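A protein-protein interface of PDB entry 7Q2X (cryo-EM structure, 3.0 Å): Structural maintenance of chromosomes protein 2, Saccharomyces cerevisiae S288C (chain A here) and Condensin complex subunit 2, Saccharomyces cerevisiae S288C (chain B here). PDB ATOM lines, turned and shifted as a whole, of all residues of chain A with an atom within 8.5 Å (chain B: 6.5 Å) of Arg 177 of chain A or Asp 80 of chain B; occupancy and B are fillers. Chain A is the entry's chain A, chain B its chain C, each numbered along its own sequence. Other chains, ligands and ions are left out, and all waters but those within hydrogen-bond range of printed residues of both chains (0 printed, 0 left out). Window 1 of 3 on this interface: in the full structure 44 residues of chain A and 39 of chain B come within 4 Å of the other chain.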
ATOM      1  N   GLN A 125       8.137   0.186   1.038  1.00  0.00           N
ATOM      2  CA  GLN A 125       8.424  -1.069   0.355  1.00  0.00           C
ATOM      3  C   GLN A 125       9.658  -0.947  -0.531  1.00  0.00           C
ATOM      4  O   GLN A 125      10.461  -1.884  -0.624  1.00  0.00           O
ATOM      5  CB  GLN A 125       7.212  -1.507  -0.470  1.00  0.00           C
ATOM      6  CG  GLN A 125       5.925  -1.642   0.327  1.00  0.00           C
ATOM      7  CD  GLN A 125       6.143  -2.255   1.696  1.00  0.00           C
ATOM      8  OE1 GLN A 125       6.359  -3.460   1.822  1.00  0.00           O
ATOM      9  NE2 GLN A 125       6.081  -1.427   2.734  1.00  0.00           N
ATOM     10  N   SER A 126       9.817   0.197  -1.201  1.00  0.00           N
ATOM     11  CA  SER A 126      10.958   0.379  -2.092  1.00  0.00           C
ATOM     12  C   SER A 126      12.271   0.251  -1.332  1.00  0.00           C
ATOM     13  O   SER A 126      13.144  -0.540  -1.707  1.00  0.00           O
ATOM     14  CB  SER A 126      10.867   1.737  -2.790  1.00  0.00           C
ATOM     15  OG  SER A 126      11.928   1.908  -3.713  1.00  0.00           O
ATOM     16  N   LEU A 128      12.663  -1.051   1.609  1.00  0.00           N
ATOM     17  CA  LEU A 128      12.725  -2.364   2.242  1.00  0.00           C
ATOM     18  C   LEU A 128      13.335  -3.399   1.304  1.00  0.00           C
ATOM     19  O   LEU A 128      14.290  -4.094   1.667  1.00  0.00           O
ATOM     20  CB  LEU A 128      11.330  -2.797   2.695  1.00  0.00           C
ATOM     21  CG  LEU A 128      10.901  -2.348   4.093  1.00  0.00           C
ATOM     22  CD1 LEU A 128       9.499  -2.846   4.412  1.00  0.00           C
ATOM     23  CD2 LEU A 128      11.895  -2.824   5.140  1.00  0.00           C
ATOM     24  N   GLN A 129      12.804  -3.508   0.083  1.00  0.00           N
ATOM     25  CA  GLN A 129      13.383  -4.449  -0.875  1.00  0.00           C
ATOM     26  C   GLN A 129      14.782  -4.022  -1.310  1.00  0.00           C
ATOM     27  O   GLN A 129      15.642  -4.875  -1.554  1.00  0.00           O
ATOM     28  CB  GLN A 129      12.470  -4.637  -2.090  1.00  0.00           C
ATOM     29  CG  GLN A 129      11.248  -5.521  -1.840  1.00  0.00           C
ATOM     30  CD  GLN A 129      10.206  -4.891  -0.945  1.00  0.00           C
ATOM     31  OE1 GLN A 129       9.636  -3.849  -1.269  1.00  0.00           O
ATOM     32  NE2 GLN A 129       9.987  -5.493   0.215  1.00  0.00           N
ATOM     33  N   LEU A 130      15.039  -2.713  -1.393  1.00  0.00           N
ATOM     34  CA  LEU A 130      16.370  -2.249  -1.768  1.00  0.00           C
ATOM     35  C   LEU A 130      17.416  -2.717  -0.766  1.00  0.00           C
ATOM     36  O   LEU A 130      18.503  -3.164  -1.151  1.00  0.00           O
ATOM     37  CB  LEU A 130      16.372  -0.723  -1.885  1.00  0.00           C
ATOM     38  CG  LEU A 130      17.595   0.011  -2.440  1.00  0.00           C
ATOM     39  CD1 LEU A 130      17.149   1.317  -3.064  1.00  0.00           C
ATOM     40  CD2 LEU A 130      18.640   0.282  -1.367  1.00  0.00           C
ATOM     41  N   GLN A 132      16.944  -5.253   1.458  1.00  0.00           N
ATOM     42  CA  GLN A 132      16.939  -6.712   1.507  1.00  0.00           C
ATOM     43  C   GLN A 132      17.758  -7.315   0.374  1.00  0.00           C
ATOM     44  O   GLN A 132      18.328  -8.401   0.533  1.00  0.00           O
ATOM     45  CB  GLN A 132      15.504  -7.236   1.463  1.00  0.00           C
ATOM     46  CG  GLN A 132      14.746  -7.090   2.771  1.00  0.00           C
ATOM     47  CD  GLN A 132      13.267  -7.388   2.624  1.00  0.00           C
ATOM     48  OE1 GLN A 132      12.418  -6.568   2.977  1.00  0.00           O
ATOM     49  NE2 GLN A 132      12.949  -8.565   2.099  1.00  0.00           N
ATOM     50  N   THR A 171      19.151 -16.659   0.582  1.00  0.00           N
ATOM     51  CA  THR A 171      17.977 -17.526   0.540  1.00  0.00           C
ATOM     52  C   THR A 171      16.727 -16.809   1.034  1.00  0.00           C
ATOM     53  O   THR A 171      15.635 -17.031   0.500  1.00  0.00           O
ATOM     54  CB  THR A 171      18.230 -18.788   1.368  1.00  0.00           C
ATOM     55  OG1 THR A 171      19.460 -19.395   0.955  1.00  0.00           O
ATOM     56  CG2 THR A 171      17.100 -19.783   1.189  1.00  0.00           C
ATOM     57  N   LYS A 172      16.861 -15.943   2.033  1.00  0.00           N
ATOM     58  CA  LYS A 172      15.725 -15.165   2.507  1.00  0.00           C
ATOM     59  C   LYS A 172      15.449 -14.065   1.476  1.00  0.00           C
ATOM     60  O   LYS A 172      16.047 -14.031   0.396  1.00  0.00           O
ATOM     61  CB  LYS A 172      15.992 -14.650   3.921  1.00  0.00           C
ATOM     62  CG  LYS A 172      14.760 -14.125   4.654  1.00  0.00           C
ATOM     63  CD  LYS A 172      14.789 -14.488   6.129  1.00  0.00           C
ATOM     64  CE  LYS A 172      14.605 -15.983   6.337  1.00  0.00           C
ATOM     65  NZ  LYS A 172      13.239 -16.436   5.951  1.00  0.00           N
ATOM     66  N   MET A 173      14.522 -13.157   1.795  1.00  0.00           N
ATOM     67  CA  MET A 173      13.863 -12.248   0.856  1.00  0.00           C
ATOM     68  C   MET A 173      12.925 -13.014  -0.072  1.00  0.00           C
ATOM     69  O   MET A 173      12.110 -12.405  -0.779  1.00  0.00           O
ATOM     70  CB  MET A 173      14.887 -11.402   0.073  1.00  0.00           C
ATOM     71  CG  MET A 173      14.522 -10.974  -1.347  1.00  0.00           C
ATOM     72  SD  MET A 173      15.877 -10.176  -2.226  1.00  0.00           S
ATOM     73  CE  MET A 173      17.128 -11.455  -2.148  1.00  0.00           C
ATOM     74  N   PHE A 174      12.946 -14.341  -0.009  1.00  0.00           N
ATOM     75  CA  PHE A 174      12.082 -15.218  -0.787  1.00  0.00           C
ATOM     76  C   PHE A 174      11.010 -15.890   0.055  1.00  0.00           C
ATOM     77  O   PHE A 174       9.883 -16.055  -0.414  1.00  0.00           O
ATOM     78  CB  PHE A 174      12.931 -16.287  -1.491  1.00  0.00           C
ATOM     79  CG  PHE A 174      12.213 -17.009  -2.595  1.00  0.00           C
ATOM     80  CD1 PHE A 174      12.140 -16.464  -3.866  1.00  0.00           C
ATOM     81  CD2 PHE A 174      11.621 -18.239  -2.365  1.00  0.00           C
ATOM     82  CE1 PHE A 174      11.485 -17.128  -4.883  1.00  0.00           C
ATOM     83  CE2 PHE A 174      10.965 -18.908  -3.379  1.00  0.00           C
ATOM     84  CZ  PHE A 174      10.896 -18.351  -4.640  1.00  0.00           C
ATOM     85  N   GLU A 175      11.332 -16.286   1.290  1.00  0.00           N
ATOM     86  CA  GLU A 175      10.345 -16.943   2.143  1.00  0.00           C
ATOM     87  C   GLU A 175       9.226 -15.983   2.528  1.00  0.00           C
ATOM     88  O   GLU A 175       8.039 -16.298   2.380  1.00  0.00           O
ATOM     89  CB  GLU A 175      11.021 -17.503   3.395  1.00  0.00           C
ATOM     90  CG  GLU A 175      12.446 -17.989   3.180  1.00  0.00           C
ATOM     91  CD  GLU A 175      12.566 -18.979   2.042  1.00  0.00           C
ATOM     92  OE1 GLU A 175      11.792 -19.959   2.016  1.00  0.00           O
ATOM     93  OE2 GLU A 175      13.440 -18.775   1.176  1.00  0.00           O
ATOM     94  N   ASP A 176       9.589 -14.799   3.031  1.00  0.00           N
ATOM     95  CA  ASP A 176       8.583 -13.791   3.344  1.00  0.00           C
ATOM     96  C   ASP A 176       7.871 -13.329   2.081  1.00  0.00           C
ATOM     97  O   ASP A 176       6.661 -13.067   2.097  1.00  0.00           O
ATOM     98  CB  ASP A 176       9.230 -12.606   4.062  1.00  0.00           C
ATOM     99  CG  ASP A 176      10.473 -12.106   3.354  1.00  0.00           C
ATOM    100  OD1 ASP A 176      10.942 -12.789   2.419  1.00  0.00           O
ATOM    101  OD2 ASP A 176      10.984 -11.030   3.733  1.00  0.00           O
ATOM    102  N   ARG A 177       8.607 -13.226   0.972  1.00  0.00           N
ATOM    103  CA  ARG A 177       7.976 -12.902  -0.300  1.00  0.00           C
ATOM    104  C   ARG A 177       7.015 -14.001  -0.728  1.00  0.00           C
ATOM    105  O   ARG A 177       5.947 -13.720  -1.280  1.00  0.00           O
ATOM    106  CB  ARG A 177       9.036 -12.662  -1.373  1.00  0.00           C
ATOM    107  CG  ARG A 177       8.463 -12.182  -2.690  1.00  0.00           C
ATOM    108  CD  ARG A 177       9.356 -11.126  -3.313  1.00  0.00           C
ATOM    109  NE  ARG A 177       9.725 -10.101  -2.345  1.00  0.00           N
ATOM    110  CZ  ARG A 177       8.938  -9.102  -1.968  1.00  0.00           C
ATOM    111  NH1 ARG A 177       7.706  -8.977  -2.433  1.00  0.00           N
ATOM    112  NH2 ARG A 177       9.396  -8.210  -1.093  1.00  0.00           N
ATOM    113  N   ARG A 178       7.377 -15.264  -0.481  1.00  0.00           N
ATOM    114  CA  ARG A 178       6.459 -16.360  -0.773  1.00  0.00           C
ATOM    115  C   ARG A 178       5.192 -16.260   0.065  1.00  0.00           C
ATOM    116  O   ARG A 178       4.088 -16.487  -0.439  1.00  0.00           O
ATOM    117  CB  ARG A 178       7.144 -17.706  -0.537  1.00  0.00           C
ATOM    118  CG  ARG A 178       7.929 -18.229  -1.727  1.00  0.00           C
ATOM    119  CD  ARG A 178       7.934 -19.755  -1.776  1.00  0.00           C
ATOM    120  NE  ARG A 178       7.846 -20.382  -0.461  1.00  0.00           N
ATOM    121  CZ  ARG A 178       8.814 -20.377   0.447  1.00  0.00           C
ATOM    122  NH1 ARG A 178       9.979 -19.793   0.215  1.00  0.00           N
ATOM    123  NH2 ARG A 178       8.610 -20.977   1.616  1.00  0.00           N
ATOM    124  N   GLU A 179       5.332 -15.929   1.352  1.00  0.00           N
ATOM    125  CA  GLU A 179       4.154 -15.785   2.204  1.00  0.00           C
ATOM    126  C   GLU A 179       3.267 -14.639   1.730  1.00  0.00           C
ATOM    127  O   GLU A 179       2.036 -14.774   1.675  1.00  0.00           O
ATOM    128  CB  GLU A 179       4.581 -15.572   3.657  1.00  0.00           C
ATOM    129  CG  GLU A 179       3.519 -15.940   4.682  1.00  0.00           C
ATOM    130  CD  GLU A 179       2.641 -14.766   5.065  1.00  0.00           C
ATOM    131  OE1 GLU A 179       3.092 -13.611   4.917  1.00  0.00           O
ATOM    132  OE2 GLU A 179       1.500 -14.998   5.517  1.00  0.00           O
ATOM    133  N   LYS A 180       3.876 -13.504   1.378  1.00  0.00           N
ATOM    134  CA  LYS A 180       3.105 -12.372   0.871  1.00  0.00           C
ATOM    135  C   LYS A 180       2.403 -12.723  -0.434  1.00  0.00           C
ATOM    136  O   LYS A 180       1.235 -12.369  -0.635  1.00  0.00           O
ATOM    137  CB  LYS A 180       4.014 -11.158   0.680  1.00  0.00           C
ATOM    138  CG  LYS A 180       4.602 -10.605   1.966  1.00  0.00           C
ATOM    139  CD  LYS A 180       3.876  -9.346   2.406  1.00  0.00           C
ATOM    140  CE  LYS A 180       4.753  -8.490   3.304  1.00  0.00           C
ATOM    141  NZ  LYS A 180       4.083  -7.214   3.681  1.00  0.00           N
ATOM    142  N   ALA A 181       3.100 -13.422  -1.333  1.00  0.00           N
ATOM    143  CA  ALA A 181       2.493 -13.831  -2.594  1.00  0.00           C
ATOM    144  C   ALA A 181       1.337 -14.793  -2.362  1.00  0.00           C
ATOM    145  O   ALA A 181       0.302 -14.695  -3.026  1.00  0.00           O
ATOM    146  CB  ALA A 181       3.545 -14.465  -3.502  1.00  0.00           C
ATOM    147  N   GLU A 182       1.495 -15.736  -1.430  1.00  0.00           N
ATOM    148  CA  GLU A 182       0.415 -16.670  -1.134  1.00  0.00           C
ATOM    149  C   GLU A 182      -0.798 -15.949  -0.561  1.00  0.00           C
ATOM    150  O   GLU A 182      -1.938 -16.256  -0.928  1.00  0.00           O
ATOM    151  CB  GLU A 182       0.903 -17.753  -0.173  1.00  0.00           C
ATOM    152  CG  GLU A 182       1.780 -18.809  -0.824  1.00  0.00           C
ATOM    153  CD  GLU A 182       1.009 -19.698  -1.779  1.00  0.00           C
ATOM    154  OE1 GLU A 182      -0.180 -19.972  -1.510  1.00  0.00           O
ATOM    155  OE2 GLU A 182       1.591 -20.125  -2.798  1.00  0.00           O
ATOM    156  N   ARG A 183      -0.576 -14.986   0.336  1.00  0.00           N
ATOM    157  CA  ARG A 183      -1.689 -14.208   0.872  1.00  0.00           C
ATOM    158  C   ARG A 183      -2.381 -13.413  -0.231  1.00  0.00           C
ATOM    159  O   ARG A 183      -3.617 -13.342  -0.287  1.00  0.00           O
ATOM    160  CB  ARG A 183      -1.196 -13.277   1.980  1.00  0.00           C
ATOM    161  CG  ARG A 183      -0.832 -13.988   3.273  1.00  0.00           C
ATOM    162  CD  ARG A 183      -1.166 -13.135   4.486  1.00  0.00           C
ATOM    163  NE  ARG A 183      -0.893 -11.722   4.253  1.00  0.00           N
ATOM    164  CZ  ARG A 183       0.278 -11.138   4.472  1.00  0.00           C
ATOM    165  NH1 ARG A 183       1.315 -11.822   4.929  1.00  0.00           N
ATOM    166  NH2 ARG A 183       0.411  -9.838   4.226  1.00  0.00           N
ATOM    167  N   THR A 184      -1.593 -12.809  -1.124  1.00  0.00           N
ATOM    168  CA  THR A 184      -2.170 -12.037  -2.220  1.00  0.00           C
ATOM    169  C   THR A 184      -2.981 -12.927  -3.152  1.00  0.00           C
ATOM    170  O   THR A 184      -4.066 -12.541  -3.598  1.00  0.00           O
ATOM    171  CB  THR A 184      -1.068 -11.317  -2.996  1.00  0.00           C
ATOM    172  OG1 THR A 184      -0.166 -10.686  -2.078  1.00  0.00           O
ATOM    173  CG2 THR A 184      -1.671 -10.262  -3.909  1.00  0.00           C
ATOM    174  N   MET A 185      -2.470 -14.121  -3.460  1.00  0.00           N
ATOM    175  CA  MET A 185      -3.213 -15.043  -4.312  1.00  0.00           C
ATOM    176  C   MET A 185      -4.480 -15.535  -3.630  1.00  0.00           C
ATOM    177  O   MET A 185      -5.505 -15.722  -4.287  1.00  0.00           O
ATOM    178  CB  MET A 185      -2.333 -16.218  -4.736  1.00  0.00           C
ATOM    179  CG  MET A 185      -1.092 -15.807  -5.498  1.00  0.00           C
ATOM    180  SD  MET A 185      -0.654 -16.989  -6.779  1.00  0.00           S
ATOM    181  CE  MET A 185       0.558 -16.044  -7.691  1.00  0.00           C
ATOM    182  N   ILE A1018       6.698 -21.796  -8.435  1.00  0.00           N
ATOM    183  CA  ILE A1018       7.048 -21.719  -7.019  1.00  0.00           C
ATOM    184  C   ILE A1018       7.492 -23.080  -6.501  1.00  0.00           C
ATOM    185  O   ILE A1018       8.443 -23.179  -5.715  1.00  0.00           O
ATOM    186  CB  ILE A1018       5.872 -21.153  -6.199  1.00  0.00           C
ATOM    187  CG1 ILE A1018       5.495 -19.756  -6.693  1.00  0.00           C
ATOM    188  CG2 ILE A1018       6.216 -21.117  -4.719  1.00  0.00           C
ATOM    189  CD1 ILE A1018       6.611 -18.742  -6.567  1.00  0.00           C
ATOM    190  N   ALA B  38       7.979  -2.880 -12.621  1.00  0.00           N
ATOM    191  CA  ALA B  38       7.358  -3.501 -11.456  1.00  0.00           C
ATOM    192  C   ALA B  38       7.872  -2.884 -10.160  1.00  0.00           C
ATOM    193  O   ALA B  38       7.109  -2.704  -9.203  1.00  0.00           O
ATOM    194  CB  ALA B  38       7.607  -5.009 -11.468  1.00  0.00           C
ATOM    195  N   LEU B  53       5.693 -10.987 -19.023  1.00  0.00           N
ATOM    196  CA  LEU B  53       6.608 -11.126 -17.895  1.00  0.00           C
ATOM    197  C   LEU B  53       6.384 -12.439 -17.159  1.00  0.00           C
ATOM    198  O   LEU B  53       7.339 -13.075 -16.703  1.00  0.00           O
ATOM    199  CB  LEU B  53       6.451  -9.943 -16.940  1.00  0.00           C
ATOM    200  CG  LEU B  53       7.420  -9.905 -15.756  1.00  0.00           C
ATOM    201  CD1 LEU B  53       8.858  -9.794 -16.237  1.00  0.00           C
ATOM    202  CD2 LEU B  53       7.075  -8.760 -14.817  1.00  0.00           C
ATOM    203  N   ALA B  75      14.721 -13.744  -9.043  1.00  0.00           N
ATOM    204  CA  ALA B  75      13.510 -14.521  -8.801  1.00  0.00           C
ATOM    205  C   ALA B  75      12.501 -13.729  -7.981  1.00  0.00           C
ATOM    206  O   ALA B  75      11.307 -13.719  -8.296  1.00  0.00           O
ATOM    207  CB  ALA B  75      13.858 -15.835  -8.102  1.00  0.00           C
ATOM    208  N   SER B  76      12.964 -13.049  -6.928  1.00  0.00           N
ATOM    209  CA  SER B  76      12.066 -12.241  -6.109  1.00  0.00           C
ATOM    210  C   SER B  76      11.497 -11.070  -6.900  1.00  0.00           C
ATOM    211  O   SER B  76      10.306 -10.756  -6.782  1.00  0.00           O
ATOM    212  CB  SER B  76      12.797 -11.745  -4.863  1.00  0.00           C
ATOM    213  OG  SER B  76      13.537 -12.789  -4.256  1.00  0.00           O
ATOM    214  N   ALA B  77      12.330 -10.409  -7.709  1.00  0.00           N
ATOM    215  CA  ALA B  77      11.835  -9.300  -8.518  1.00  0.00           C
ATOM    216  C   ALA B  77      10.786  -9.771  -9.521  1.00  0.00           C
ATOM    217  O   ALA B  77       9.745  -9.122  -9.699  1.00  0.00           O
ATOM    218  CB  ALA B  77      12.997  -8.614  -9.236  1.00  0.00           C
ATOM    219  N   THR B  78      11.039 -10.905 -10.178  1.00  0.00           N
ATOM    220  CA  THR B  78      10.082 -11.432 -11.144  1.00  0.00           C
ATOM    221  C   THR B  78       8.799 -11.878 -10.458  1.00  0.00           C
ATOM    222  O   THR B  78       7.706 -11.710 -11.008  1.00  0.00           O
ATOM    223  CB  THR B  78      10.706 -12.587 -11.923  1.00  0.00           C
ATOM    224  OG1 THR B  78      12.055 -12.255 -12.271  1.00  0.00           O
ATOM    225  CG2 THR B  78       9.923 -12.843 -13.198  1.00  0.00           C
ATOM    226  N   LEU B  79       8.910 -12.451  -9.258  1.00  0.00           N
ATOM    227  CA  LEU B  79       7.718 -12.823  -8.505  1.00  0.00           C
ATOM    228  C   LEU B  79       6.899 -11.594  -8.137  1.00  0.00           C
ATOM    229  O   LEU B  79       5.667 -11.614  -8.225  1.00  0.00           O
ATOM    230  CB  LEU B  79       8.109 -13.607  -7.253  1.00  0.00           C
ATOM    231  CG  LEU B  79       6.961 -14.214  -6.443  1.00  0.00           C
ATOM    232  CD1 LEU B  79       6.020 -14.996  -7.347  1.00  0.00           C
ATOM    233  CD2 LEU B  79       7.500 -15.098  -5.330  1.00  0.00           C
ATOM    234  N   ASP B  80       7.566 -10.513  -7.724  1.00  0.00           N
ATOM    235  CA  ASP B  80       6.855  -9.273  -7.430  1.00  0.00           C
ATOM    236  C   ASP B  80       6.137  -8.748  -8.666  1.00  0.00           C
ATOM    237  O   ASP B  80       4.974  -8.327  -8.592  1.00  0.00           O
ATOM    238  CB  ASP B  80       7.827  -8.222  -6.897  1.00  0.00           C
ATOM    239  CG  ASP B  80       7.941  -8.245  -5.390  1.00  0.00           C
ATOM    240  OD1 ASP B  80       6.901  -8.408  -4.717  1.00  0.00           O
ATOM    241  OD2 ASP B  80       9.068  -8.096  -4.876  1.00  0.00           O
ATOM    242  N   GLY B  81       6.818  -8.766  -9.815  1.00  0.00           N
ATOM    243  CA  GLY B  81       6.174  -8.342 -11.048  1.00  0.00           C
ATOM    244  C   GLY B  81       4.975  -9.200 -11.402  1.00  0.00           C
ATOM    245  O   GLY B  81       3.941  -8.690 -11.841  1.00  0.00           O
ATOM    246  N   CYS B  82       5.096 -10.516 -11.212  1.00  0.00           N
ATOM    247  CA  CYS B  82       3.987 -11.417 -11.505  1.00  0.00           C
ATOM    248  C   CYS B  82       2.803 -11.160 -10.582  1.00  0.00           C
ATOM    249  O   CYS B  82       1.650 -11.180 -11.024  1.00  0.00           O
ATOM    250  CB  CYS B  82       4.446 -12.871 -11.400  1.00  0.00           C
ATOM    251  SG  CYS B  82       5.611 -13.376 -12.686  1.00  0.00           S
ATOM    252  N   ILE B  83       3.064 -10.921  -9.294  1.00  0.00           N
ATOM    253  CA  ILE B  83       1.975 -10.618  -8.364  1.00  0.00           C
ATOM    254  C   ILE B  83       1.292  -9.313  -8.749  1.00  0.00           C
ATOM    255  O   ILE B  83       0.060  -9.207  -8.715  1.00  0.00           O
ATOM    256  CB  ILE B  83       2.483 -10.579  -6.910  1.00  0.00           C
ATOM    257  CG1 ILE B  83       3.211 -11.874  -6.543  1.00  0.00           C
ATOM    258  CG2 ILE B  83       1.333 -10.332  -5.950  1.00  0.00           C
ATOM    259  CD1 ILE B  83       2.484 -13.128  -6.961  1.00  0.00           C
ATOM    260  N   LYS B  84       2.078  -8.294  -9.110  1.00  0.00           N
ATOM    261  CA  LYS B  84       1.482  -7.024  -9.520  1.00  0.00           C
ATOM    262  C   LYS B  84       0.629  -7.192 -10.772  1.00  0.00           C
ATOM    263  O   LYS B  84      -0.485  -6.659 -10.852  1.00  0.00           O
ATOM    264  CB  LYS B  84       2.574  -5.978  -9.745  1.00  0.00           C
ATOM    265  CG  LYS B  84       3.283  -5.544  -8.474  1.00  0.00           C
ATOM    266  CD  LYS B  84       2.432  -4.573  -7.672  1.00  0.00           C
ATOM    267  CE  LYS B  84       3.146  -4.127  -6.405  1.00  0.00           C
ATOM    268  NZ  LYS B  84       4.621  -4.058  -6.594  1.00  0.00           N
ATOM    269  N   ILE B  85       1.131  -7.945 -11.755  1.00  0.00           N
ATOM    270  CA  ILE B  85       0.376  -8.176 -12.984  1.00  0.00           C
ATOM    271  C   ILE B  85      -0.903  -8.949 -12.687  1.00  0.00           C
ATOM    272  O   ILE B  85      -1.969  -8.650 -13.238  1.00  0.00           O
ATOM    273  CB  ILE B  85       1.255  -8.903 -14.019  1.00  0.00           C
ATOM    274  CG1 ILE B  85       2.311  -7.950 -14.578  1.00  0.00           C
ATOM    275  CG2 ILE B  85       0.407  -9.474 -15.145  1.00  0.00           C
ATOM    276  CD1 ILE B  85       3.275  -8.604 -15.541  1.00  0.00           C
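NE2 of Gln 129 of chain A sits close to NH2 of Arg 177 of chain A (3.1 Å). The backbone carbonyl oxygen (O) of Lys 180 of chain A is in hydrogen-bond range of the side-chain hydroxyl (OG1) of Thr 184 of chain A (2.6 Å).
Gln 132 of chain A touches none of the printed residues of chain B. Arg 177 of chain A touches just these residues of chain B: Ser 76 and Asp 80. Lys 180 of chain A touches none of the printed residues of chain B. Printed residues of chain B within 4 Å of Ile 1018 of chain A: Leu 79 (3.9 Å). Asp 80 of chain B touches just one residue of chain A: Arg 177. Of the printed residues of chain A, Ile 83 of chain B touches Ala 181, Thr 184 and Met 185. The nearest residue of chain B that does not touch Arg 177 of chain A is Leu 79 of chain B (4.05 Å).
NH1 of Arg 177 of chain A lies within salt-bridge range of OD1 of Asp 80 of chain B, at 2.5 Å.
Hydrophobic or aromatic side chains of chain A that line the printed part of chain B: Met 173, Phe 174, Ala 181, Met 185 and Ile 1018. Of the 13 printed residues of chain B, 4 touch a printed residue of chain A. Printed residues of chain B that touch a printed residue of chain A: Ser 76, Leu 79, Asp 80 and Ile 83. Hydrophobic or aromatic side chains of chain B within 4 Å of the printed part of chain A: Leu 79 and Ile 83. Among the printed residues, 8 pairs touch across the chains.
Among the printed residues, merely in contact across the chains: Met 173 of chain A with Ser 76 of chain B (3.6 Å), Phe 174 of chain A with Ser 76 of chain B (3.95 Å), Arg 177 of chain A with Ser 76 of chain B (3.6 Å), Ala 181 of chain A with Ile 83 of chain B (3.9 Å), Thr 184 of chain A with Ile 83 of chain B (3.6 Å), Met 185 of chain A with Ile 83 of chain B (3.6 Å) and Ile 1018 of chain A with Leu 79 of chain B (3.9 Å).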
